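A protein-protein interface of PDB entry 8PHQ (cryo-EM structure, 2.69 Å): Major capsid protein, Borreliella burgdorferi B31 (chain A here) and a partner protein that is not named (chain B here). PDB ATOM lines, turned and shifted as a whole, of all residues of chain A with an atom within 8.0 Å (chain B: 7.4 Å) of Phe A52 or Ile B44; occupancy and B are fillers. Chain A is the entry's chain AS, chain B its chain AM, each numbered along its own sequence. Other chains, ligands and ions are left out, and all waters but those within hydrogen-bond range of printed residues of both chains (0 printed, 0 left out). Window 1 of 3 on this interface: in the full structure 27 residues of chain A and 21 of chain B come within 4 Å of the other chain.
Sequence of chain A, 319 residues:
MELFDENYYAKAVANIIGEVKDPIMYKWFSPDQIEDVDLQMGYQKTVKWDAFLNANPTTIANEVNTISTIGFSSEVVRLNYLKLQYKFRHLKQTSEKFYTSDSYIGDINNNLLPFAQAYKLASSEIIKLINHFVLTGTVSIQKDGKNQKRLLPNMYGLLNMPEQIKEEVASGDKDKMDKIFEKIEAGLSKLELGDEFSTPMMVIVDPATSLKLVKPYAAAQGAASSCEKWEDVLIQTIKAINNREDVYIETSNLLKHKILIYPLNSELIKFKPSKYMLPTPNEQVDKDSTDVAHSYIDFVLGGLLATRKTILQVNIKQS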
ATOM      1  N   ASP A  50      25.459  14.604  -4.036  1.00  0.00           N
ATOM      2  CA  ASP A  50      25.900  15.704  -4.880  1.00  0.00           C
ATOM      3  C   ASP A  50      24.812  16.766  -4.965  1.00  0.00           C
ATOM      4  O   ASP A  50      23.633  16.500  -4.722  1.00  0.00           O
ATOM      5  CB  ASP A  50      26.265  15.219  -6.289  1.00  0.00           C
ATOM      6  CG  ASP A  50      27.107  13.960  -6.270  1.00  0.00           C
ATOM      7  OD1 ASP A  50      28.224  13.999  -5.713  1.00  0.00           O
ATOM      8  OD2 ASP A  50      26.651  12.929  -6.808  1.00  0.00           O
ATOM      9  N   ALA A  51      25.228  17.979  -5.316  1.00  0.00           N
ATOM     10  CA  ALA A  51      24.325  19.105  -5.494  1.00  0.00           C
ATOM     11  C   ALA A  51      24.639  19.800  -6.809  1.00  0.00           C
ATOM     12  O   ALA A  51      25.770  19.753  -7.299  1.00  0.00           O
ATOM     13  CB  ALA A  51      24.430  20.103  -4.339  1.00  0.00           C
ATOM     14  N   PHE A  52      23.627  20.448  -7.381  1.00  0.00           N
ATOM     15  CA  PHE A  52      23.788  21.116  -8.662  1.00  0.00           C
ATOM     16  C   PHE A  52      22.909  22.356  -8.704  1.00  0.00           C
ATOM     17  O   PHE A  52      21.927  22.472  -7.969  1.00  0.00           O
ATOM     18  CB  PHE A  52      23.458  20.172  -9.826  1.00  0.00           C
ATOM     19  CG  PHE A  52      22.126  19.487  -9.699  1.00  0.00           C
ATOM     20  CD1 PHE A  52      20.949  20.165  -9.968  1.00  0.00           C
ATOM     21  CD2 PHE A  52      22.052  18.165  -9.303  1.00  0.00           C
ATOM     22  CE1 PHE A  52      19.728  19.534  -9.852  1.00  0.00           C
ATOM     23  CE2 PHE A  52      20.833  17.530  -9.183  1.00  0.00           C
ATOM     24  CZ  PHE A  52      19.670  18.216  -9.457  1.00  0.00           C
ATOM     25  N   LEU A  53      23.273  23.282  -9.585  1.00  0.00           N
ATOM     26  CA  LEU A  53      22.536  24.522  -9.781  1.00  0.00           C
ATOM     27  C   LEU A  53      21.576  24.356 -10.951  1.00  0.00           C
ATOM     28  O   LEU A  53      21.980  23.919 -12.033  1.00  0.00           O
ATOM     29  CB  LEU A  53      23.493  25.687 -10.041  1.00  0.00           C
ATOM     30  CG  LEU A  53      24.560  25.956  -8.978  1.00  0.00           C
ATOM     31  CD1 LEU A  53      25.346  27.209  -9.316  1.00  0.00           C
ATOM     32  CD2 LEU A  53      23.936  26.075  -7.603  1.00  0.00           C
ATOM     33  N   ASN A  54      20.307  24.702 -10.733  1.00  0.00           N
ATOM     34  CA  ASN A  54      19.289  24.545 -11.765  1.00  0.00           C
ATOM     35  C   ASN A  54      19.165  25.753 -12.680  1.00  0.00           C
ATOM     36  O   ASN A  54      18.784  25.599 -13.846  1.00  0.00           O
ATOM     37  CB  ASN A  54      17.927  24.258 -11.130  1.00  0.00           C
ATOM     38  CG  ASN A  54      17.794  22.828 -10.665  1.00  0.00           C
ATOM     39  OD1 ASN A  54      17.875  21.897 -11.462  1.00  0.00           O
ATOM     40  ND2 ASN A  54      17.583  22.644  -9.368  1.00  0.00           N
ATOM     41  N   ALA A  55      19.469  26.950 -12.187  1.00  0.00           N
ATOM     42  CA  ALA A  55      19.331  28.161 -12.981  1.00  0.00           C
ATOM     43  C   ALA A  55      20.299  29.208 -12.446  1.00  0.00           C
ATOM     44  O   ALA A  55      20.978  28.997 -11.438  1.00  0.00           O
ATOM     45  CB  ALA A  55      17.888  28.670 -12.964  1.00  0.00           C
ATOM     46  N   THR A  69      16.386  27.454  -7.736  1.00  0.00           N
ATOM     47  CA  THR A  69      16.524  26.331  -6.823  1.00  0.00           C
ATOM     48  C   THR A  69      17.839  25.592  -7.040  1.00  0.00           C
ATOM     49  O   THR A  69      18.454  25.658  -8.107  1.00  0.00           O
ATOM     50  CB  THR A  69      15.356  25.352  -6.979  1.00  0.00           C
ATOM     51  OG1 THR A  69      15.334  24.842  -8.316  1.00  0.00           O
ATOM     52  CG2 THR A  69      14.038  26.042  -6.681  1.00  0.00           C
ATOM     53  N   ILE A  70      18.257  24.882  -5.995  1.00  0.00           N
ATOM     54  CA  ILE A  70      19.412  23.993  -6.028  1.00  0.00           C
ATOM     55  C   ILE A  70      18.914  22.578  -5.777  1.00  0.00           C
ATOM     56  O   ILE A  70      18.269  22.315  -4.755  1.00  0.00           O
ATOM     57  CB  ILE A  70      20.473  24.388  -4.988  1.00  0.00           C
ATOM     58  CG1 ILE A  70      21.015  25.787  -5.274  1.00  0.00           C
ATOM     59  CG2 ILE A  70      21.592  23.362  -4.942  1.00  0.00           C
ATOM     60  CD1 ILE A  70      22.032  26.252  -4.262  1.00  0.00           C
ATOM     61  N   GLY A  71      19.212  21.669  -6.705  1.00  0.00           N
ATOM     62  CA  GLY A  71      18.807  20.287  -6.574  1.00  0.00           C
ATOM     63  C   GLY A  71      19.867  19.426  -5.908  1.00  0.00           C
ATOM     64  O   GLY A  71      20.963  19.873  -5.577  1.00  0.00           O
ATOM     65  N   PHE A  72      19.516  18.157  -5.714  1.00  0.00           N
ATOM     66  CA  PHE A  72      20.405  17.195  -5.083  1.00  0.00           C
ATOM     67  C   PHE A  72      20.298  15.859  -5.804  1.00  0.00           C
ATOM     68  O   PHE A  72      19.238  15.496  -6.317  1.00  0.00           O
ATOM     69  CB  PHE A  72      20.075  17.028  -3.597  1.00  0.00           C
ATOM     70  CG  PHE A  72      20.298  18.271  -2.791  1.00  0.00           C
ATOM     71  CD1 PHE A  72      21.577  18.747  -2.568  1.00  0.00           C
ATOM     72  CD2 PHE A  72      19.228  18.978  -2.273  1.00  0.00           C
ATOM     73  CE1 PHE A  72      21.785  19.895  -1.831  1.00  0.00           C
ATOM     74  CE2 PHE A  72      19.430  20.127  -1.538  1.00  0.00           C
ATOM     75  CZ  PHE A  72      20.709  20.586  -1.319  1.00  0.00           C
ATOM     76  N   SER A  73      21.413  15.133  -5.840  1.00  0.00           N
ATOM     77  CA  SER A  73      21.483  13.846  -6.516  1.00  0.00           C
ATOM     78  C   SER A  73      22.271  12.870  -5.655  1.00  0.00           C
ATOM     79  O   SER A  73      23.062  13.266  -4.796  1.00  0.00           O
ATOM     80  CB  SER A  73      22.122  13.975  -7.904  1.00  0.00           C
ATOM     81  OG  SER A  73      22.017  12.763  -8.628  1.00  0.00           O
ATOM     82  N   SER A  74      22.048  11.579  -5.896  1.00  0.00           N
ATOM     83  CA  SER A  74      22.688  10.532  -5.114  1.00  0.00           C
ATOM     84  C   SER A  74      23.142   9.405  -6.028  1.00  0.00           C
ATOM     85  O   SER A  74      22.626   9.223  -7.133  1.00  0.00           O
ATOM     86  CB  SER A  74      21.752   9.978  -4.033  1.00  0.00           C
ATOM     87  OG  SER A  74      20.589   9.411  -4.608  1.00  0.00           O
ATOM     88  N   LYS B  23      12.240   7.809 -12.414  1.00  0.00           N
ATOM     89  CA  LYS B  23      12.946   9.050 -12.117  1.00  0.00           C
ATOM     90  C   LYS B  23      14.304   8.777 -11.479  1.00  0.00           C
ATOM     91  O   LYS B  23      15.327   9.314 -11.921  1.00  0.00           O
ATOM     92  CB  LYS B  23      12.089   9.940 -11.213  1.00  0.00           C
ATOM     93  CG  LYS B  23      11.488   9.233 -10.012  1.00  0.00           C
ATOM     94  CD  LYS B  23      10.953  10.228  -8.998  1.00  0.00           C
ATOM     95  CE  LYS B  23      12.021  11.228  -8.594  1.00  0.00           C
ATOM     96  NZ  LYS B  23      11.573  12.087  -7.466  1.00  0.00           N
ATOM     97  N   ASP B  37      32.162  18.783 -11.402  1.00  0.00           N
ATOM     98  CA  ASP B  37      32.056  20.096 -12.029  1.00  0.00           C
ATOM     99  C   ASP B  37      30.813  20.750 -11.437  1.00  0.00           C
ATOM    100  O   ASP B  37      30.037  20.106 -10.725  1.00  0.00           O
ATOM    101  CB  ASP B  37      31.958  20.011 -13.556  1.00  0.00           C
ATOM    102  CG  ASP B  37      32.210  21.343 -14.234  1.00  0.00           C
ATOM    103  OD1 ASP B  37      32.525  22.322 -13.528  1.00  0.00           O
ATOM    104  OD2 ASP B  37      32.096  21.411 -15.476  1.00  0.00           O
ATOM    105  N   PHE B  38      30.628  22.036 -11.734  1.00  0.00           N
ATOM    106  CA  PHE B  38      29.430  22.746 -11.303  1.00  0.00           C
ATOM    107  C   PHE B  38      28.582  23.224 -12.473  1.00  0.00           C
ATOM    108  O   PHE B  38      27.615  23.964 -12.260  1.00  0.00           O
ATOM    109  CB  PHE B  38      29.790  23.933 -10.403  1.00  0.00           C
ATOM    110  CG  PHE B  38      30.331  25.121 -11.145  1.00  0.00           C
ATOM    111  CD1 PHE B  38      31.574  25.074 -11.754  1.00  0.00           C
ATOM    112  CD2 PHE B  38      29.590  26.288 -11.238  1.00  0.00           C
ATOM    113  CE1 PHE B  38      32.067  26.169 -12.435  1.00  0.00           C
ATOM    114  CE2 PHE B  38      30.078  27.384 -11.920  1.00  0.00           C
ATOM    115  CZ  PHE B  38      31.318  27.325 -12.519  1.00  0.00           C
ATOM    116  N   ARG B  39      28.908  22.823 -13.699  1.00  0.00           N
ATOM    117  CA  ARG B  39      28.179  23.252 -14.883  1.00  0.00           C
ATOM    118  C   ARG B  39      27.515  22.061 -15.557  1.00  0.00           C
ATOM    119  O   ARG B  39      28.122  20.994 -15.692  1.00  0.00           O
ATOM    120  CB  ARG B  39      29.102  23.967 -15.873  1.00  0.00           C
ATOM    121  CG  ARG B  39      29.781  25.202 -15.307  1.00  0.00           C
ATOM    122  CD  ARG B  39      30.765  25.795 -16.302  1.00  0.00           C
ATOM    123  NE  ARG B  39      31.848  24.875 -16.627  1.00  0.00           N
ATOM    124  CZ  ARG B  39      33.133  25.132 -16.427  1.00  0.00           C
ATOM    125  NH1 ARG B  39      33.534  26.278 -15.906  1.00  0.00           N
ATOM    126  NH2 ARG B  39      34.038  24.217 -16.762  1.00  0.00           N
ATOM    127  N   ASP B  40      26.263  22.256 -15.977  1.00  0.00           N
ATOM    128  CA  ASP B  40      25.486  21.243 -16.695  1.00  0.00           C
ATOM    129  C   ASP B  40      25.358  19.949 -15.894  1.00  0.00           C
ATOM    130  O   ASP B  40      25.369  18.849 -16.450  1.00  0.00           O
ATOM    131  CB  ASP B  40      26.079  20.966 -18.077  1.00  0.00           C
ATOM    132  CG  ASP B  40      25.986  22.164 -18.998  1.00  0.00           C
ATOM    133  OD1 ASP B  40      25.468  23.209 -18.557  1.00  0.00           O
ATOM    134  OD2 ASP B  40      26.429  22.060 -20.161  1.00  0.00           O
ATOM    135  N   GLN B  41      25.226  20.078 -14.577  1.00  0.00           N
ATOM    136  CA  GLN B  41      24.983  18.932 -13.715  1.00  0.00           C
ATOM    137  C   GLN B  41      23.505  18.713 -13.425  1.00  0.00           C
ATOM    138  O   GLN B  41      23.163  17.752 -12.729  1.00  0.00           O
ATOM    139  CB  GLN B  41      25.749  19.090 -12.398  1.00  0.00           C
ATOM    140  CG  GLN B  41      27.215  19.443 -12.567  1.00  0.00           C
ATOM    141  CD  GLN B  41      28.040  18.274 -13.065  1.00  0.00           C
ATOM    142  OE1 GLN B  41      28.112  17.229 -12.419  1.00  0.00           O
ATOM    143  NE2 GLN B  41      28.668  18.444 -14.223  1.00  0.00           N
ATOM    144  N   ASN B  42      22.626  19.572 -13.939  1.00  0.00           N
ATOM    145  CA  ASN B  42      21.197  19.484 -13.675  1.00  0.00           C
ATOM    146  C   ASN B  42      20.417  18.833 -14.807  1.00  0.00           C
ATOM    147  O   ASN B  42      19.190  18.728 -14.715  1.00  0.00           O
ATOM    148  CB  ASN B  42      20.629  20.879 -13.395  1.00  0.00           C
ATOM    149  CG  ASN B  42      20.701  21.791 -14.602  1.00  0.00           C
ATOM    150  OD1 ASN B  42      21.781  22.070 -15.121  1.00  0.00           O
ATOM    151  ND2 ASN B  42      19.548  22.270 -15.050  1.00  0.00           N
ATOM    152  N   LEU B  43      21.090  18.395 -15.870  1.00  0.00           N
ATOM    153  CA  LEU B  43      20.416  17.783 -17.016  1.00  0.00           C
ATOM    154  C   LEU B  43      20.281  16.277 -16.785  1.00  0.00           C
ATOM    155  O   LEU B  43      20.862  15.444 -17.481  1.00  0.00           O
ATOM    156  CB  LEU B  43      21.170  18.090 -18.304  1.00  0.00           C
ATOM    157  CG  LEU B  43      21.126  19.522 -18.845  1.00  0.00           C
ATOM    158  CD1 LEU B  43      22.105  20.429 -18.118  1.00  0.00           C
ATOM    159  CD2 LEU B  43      21.405  19.531 -20.337  1.00  0.00           C
ATOM    160  N   ILE B  44      19.487  15.938 -15.769  1.00  0.00           N
ATOM    161  CA  ILE B  44      19.243  14.554 -15.394  1.00  0.00           C
ATOM    162  C   ILE B  44      17.747  14.347 -15.195  1.00  0.00           C
ATOM    163  O   ILE B  44      16.994  15.285 -14.926  1.00  0.00           O
ATOM    164  CB  ILE B  44      20.019  14.147 -14.122  1.00  0.00           C
ATOM    165  CG1 ILE B  44      19.744  15.137 -12.990  1.00  0.00           C
ATOM    166  CG2 ILE B  44      21.508  14.060 -14.412  1.00  0.00           C
ATOM    167  CD1 ILE B  44      20.478  14.816 -11.709  1.00  0.00           C
ATOM    168  N   PHE B  45      17.325  13.088 -15.332  1.00  0.00           N
ATOM    169  CA  PHE B  45      15.909  12.760 -15.208  1.00  0.00           C
ATOM    170  C   PHE B  45      15.428  12.860 -13.767  1.00  0.00           C
ATOM    171  O   PHE B  45      14.253  13.163 -13.528  1.00  0.00           O
ATOM    172  CB  PHE B  45      15.652  11.359 -15.761  1.00  0.00           C
ATOM    173  CG  PHE B  45      14.216  11.095 -16.105  1.00  0.00           C
ATOM    174  CD1 PHE B  45      13.519  11.953 -16.937  1.00  0.00           C
ATOM    175  CD2 PHE B  45      13.565   9.979 -15.607  1.00  0.00           C
ATOM    176  CE1 PHE B  45      12.197  11.709 -17.258  1.00  0.00           C
ATOM    177  CE2 PHE B  45      12.245   9.729 -15.925  1.00  0.00           C
ATOM    178  CZ  PHE B  45      11.561  10.595 -16.752  1.00  0.00           C
ATOM    179  N   SER B  46      16.309  12.614 -12.797  1.00  0.00           N
ATOM    180  CA  SER B  46      15.922  12.660 -11.392  1.00  0.00           C
ATOM    181  C   SER B  46      15.702  14.078 -10.879  1.00  0.00           C
ATOM    182  O   SER B  46      15.221  14.240  -9.754  1.00  0.00           O
ATOM    183  CB  SER B  46      16.979  11.961 -10.537  1.00  0.00           C
ATOM    184  OG  SER B  46      18.257  12.541 -10.727  1.00  0.00           O
ATOM    185  N   ASN B  47      16.041  15.097 -11.664  1.00  0.00           N
ATOM    186  CA  ASN B  47      15.851  16.487 -11.257  1.00  0.00           C
ATOM    187  C   ASN B  47      14.361  16.800 -11.244  1.00  0.00           C
ATOM    188  O   ASN B  47      13.765  17.091 -12.281  1.00  0.00           O
ATOM    189  CB  ASN B  47      16.598  17.419 -12.204  1.00  0.00           C
ATOM    190  CG  ASN B  47      16.681  18.836 -11.681  1.00  0.00           C
ATOM    191  OD1 ASN B  47      16.245  19.126 -10.567  1.00  0.00           O
ATOM    192  ND2 ASN B  47      17.235  19.732 -12.488  1.00  0.00           N
ATOM    193  N   SER B  48      13.755  16.753 -10.063  1.00  0.00           N
ATOM    194  CA  SER B  48      12.324  16.960  -9.907  1.00  0.00           C
ATOM    195  C   SER B  48      12.028  18.400  -9.504  1.00  0.00           C
ATOM    196  O   SER B  48      12.921  19.177  -9.158  1.00  0.00           O
ATOM    197  CB  SER B  48      11.751  15.985  -8.874  1.00  0.00           C
ATOM    198  OG  SER B  48      12.410  16.119  -7.629  1.00  0.00           O
ATOM    199  N   TYR B  69       5.315  10.900 -14.859  1.00  0.00           N
ATOM    200  CA  TYR B  69       6.367  11.800 -14.399  1.00  0.00           C
ATOM    201  C   TYR B  69       6.831  12.730 -15.515  1.00  0.00           C
ATOM    202  O   TYR B  69       7.093  12.291 -16.638  1.00  0.00           O
ATOM    203  CB  TYR B  69       7.546  10.987 -13.868  1.00  0.00           C
ATOM    204  CG  TYR B  69       8.698  11.816 -13.351  1.00  0.00           C
ATOM    205  CD1 TYR B  69       8.532  12.681 -12.281  1.00  0.00           C
ATOM    206  CD2 TYR B  69       9.954  11.728 -13.932  1.00  0.00           C
ATOM    207  CE1 TYR B  69       9.585  13.437 -11.807  1.00  0.00           C
ATOM    208  CE2 TYR B  69      11.011  12.479 -13.467  1.00  0.00           C
ATOM    209  CZ  TYR B  69      10.822  13.332 -12.404  1.00  0.00           C
ATOM    210  OH  TYR B  69      11.874  14.082 -11.938  1.00  0.00           O
ATOM    211  N   LYS B  70       6.934  14.022 -15.190  1.00  0.00           N
ATOM    212  CA  LYS B  70       7.392  15.058 -16.121  1.00  0.00           C
ATOM    213  C   LYS B  70       6.558  15.091 -17.398  1.00  0.00           C
ATOM    214  O   LYS B  70       7.088  15.206 -18.503  1.00  0.00           O
ATOM    215  CB  LYS B  70       8.876  14.893 -16.455  1.00  0.00           C
ATOM    216  CG  LYS B  70       9.815  15.341 -15.354  1.00  0.00           C
ATOM    217  CD  LYS B  70      11.251  15.353 -15.840  1.00  0.00           C
ATOM    218  CE  LYS B  70      12.187  15.889 -14.776  1.00  0.00           C
ATOM    219  NZ  LYS B  70      11.764  17.227 -14.283  1.00  0.00           N
ATOM    220  N   TYR B 120      11.881  21.506 -16.419  1.00  0.00           N
ATOM    221  CA  TYR B 120      12.193  20.578 -17.497  1.00  0.00           C
ATOM    222  C   TYR B 120      11.058  19.579 -17.670  1.00  0.00           C
ATOM    223  O   TYR B 120      10.625  18.949 -16.700  1.00  0.00           O
ATOM    224  CB  TYR B 120      13.505  19.851 -17.206  1.00  0.00           C
ATOM    225  CG  TYR B 120      14.727  20.712 -17.417  1.00  0.00           C
ATOM    226  CD1 TYR B 120      15.166  21.025 -18.694  1.00  0.00           C
ATOM    227  CD2 TYR B 120      15.426  21.233 -16.337  1.00  0.00           C
ATOM    228  CE1 TYR B 120      16.276  21.817 -18.891  1.00  0.00           C
ATOM    229  CE2 TYR B 120      16.536  22.028 -16.525  1.00  0.00           C
ATOM    230  CZ  TYR B 120      16.957  22.317 -17.804  1.00  0.00           C
ATOM    231  OH  TYR B 120      18.065  23.108 -17.997  1.00  0.00           O
ATOM    232  N   LEU B 166      18.408  12.494 -23.176  1.00  0.00           N
ATOM    233  CA  LEU B 166      18.821  11.645 -22.067  1.00  0.00           C
ATOM    234  C   LEU B 166      18.897  10.177 -22.453  1.00  0.00           C
ATOM    235  O   LEU B 166      19.645   9.418 -21.831  1.00  0.00           O
ATOM    236  CB  LEU B 166      17.855  11.804 -20.888  1.00  0.00           C
ATOM    237  CG  LEU B 166      17.677  13.212 -20.320  1.00  0.00           C
ATOM    238  CD1 LEU B 166      16.896  13.166 -19.021  1.00  0.00           C
ATOM    239  CD2 LEU B 166      19.024  13.878 -20.110  1.00  0.00           C
ATOM    240  N   LEU B 170      14.208   9.382 -25.021  1.00  0.00           N
ATOM    241  CA  LEU B 170      13.871  10.351 -23.985  1.00  0.00           C
ATOM    242  C   LEU B 170      14.552  11.685 -24.272  1.00  0.00           C
ATOM    243  O   LEU B 170      15.786  11.775 -24.276  1.00  0.00           O
ATOM    244  CB  LEU B 170      14.273   9.828 -22.606  1.00  0.00           C
ATOM    245  CG  LEU B 170      13.909  10.706 -21.410  1.00  0.00           C
ATOM    246  CD1 LEU B 170      12.404  10.889 -21.324  1.00  0.00           C
ATOM    247  CD2 LEU B 170      14.450  10.102 -20.126  1.00  0.00           C
ATOM    248  N   ILE B 172      14.211  15.942 -23.115  1.00  0.00           N
ATOM    249  CA  ILE B 172      13.626  16.911 -22.199  1.00  0.00           C
ATOM    250  C   ILE B 172      13.958  18.310 -22.691  1.00  0.00           C
ATOM    251  O   ILE B 172      14.898  18.513 -23.465  1.00  0.00           O
ATOM    252  CB  ILE B 172      14.102  16.714 -20.742  1.00  0.00           C
ATOM    253  CG1 ILE B 172      15.607  16.943 -20.624  1.00  0.00           C
ATOM    254  CG2 ILE B 172      13.719  15.333 -20.234  1.00  0.00           C
ATOM    255  CD1 ILE B 172      16.093  17.023 -19.194  1.00  0.00           C
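OD1 of Asn A54 lies within hydrogen-bond range of ND2 of Asn B47 (2.5 Å).
The side-chain amide nitrogen (NE2) of Gln B41 lies within hydrogen-bond range of the backbone carbonyl oxygen (O) of Arg B39, 3.0 Å away.
ND2 of Asn B42 lies close to OH of Tyr B120, at 3.4 Å.
ND2 of Asn A54 sits at hydrogen-bond distance from OG1 of Thr A69 (3.3 Å).
N of Gly A71 lies within hydrogen-bond range of O of Phe A52, 3.1 Å away.
ND2 of Asn B47 sits at hydrogen-bond distance from O of Asn B42.
The side-chain amide nitrogen (ND2) of Asn A54 lies close to the backbone NH (N) of Gly A71, 3.3 Å away.
Among the printed residues, merely in contact across the chains: Phe A52 with Gln B41 (3.6 Å), Phe A52 with Asn B42 (3.5 Å), Phe A52 with Ile B44 (3.7 Å), Phe A52 with Asn B47 (3.6 Å), Leu A53 with Asn B42 (3.6 Å) and Asn A54 with Asn B42 (3.5 Å).
Hydrophobic or aromatic side chains of chain A within 4 Å of the printed part of chain B: Phe A52.
Among the printed residues, no Asp or Glu carboxylate lies within 4 Å of a Lys or Arg side-chain nitrogen of the other chain.
Of the printed residues of chain B, Asn A54 touches Asn B42 and Asn B47.
Printed residues of chain A within 4 Å of Gln B41: Phe A52 (3.6 Å).
Printed residues of chain A within 4 Å of Ile B44: Phe A52.
The nearest printed residue of chain A that does not touch Ile B44 is Ser A73 (4.01 Å).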
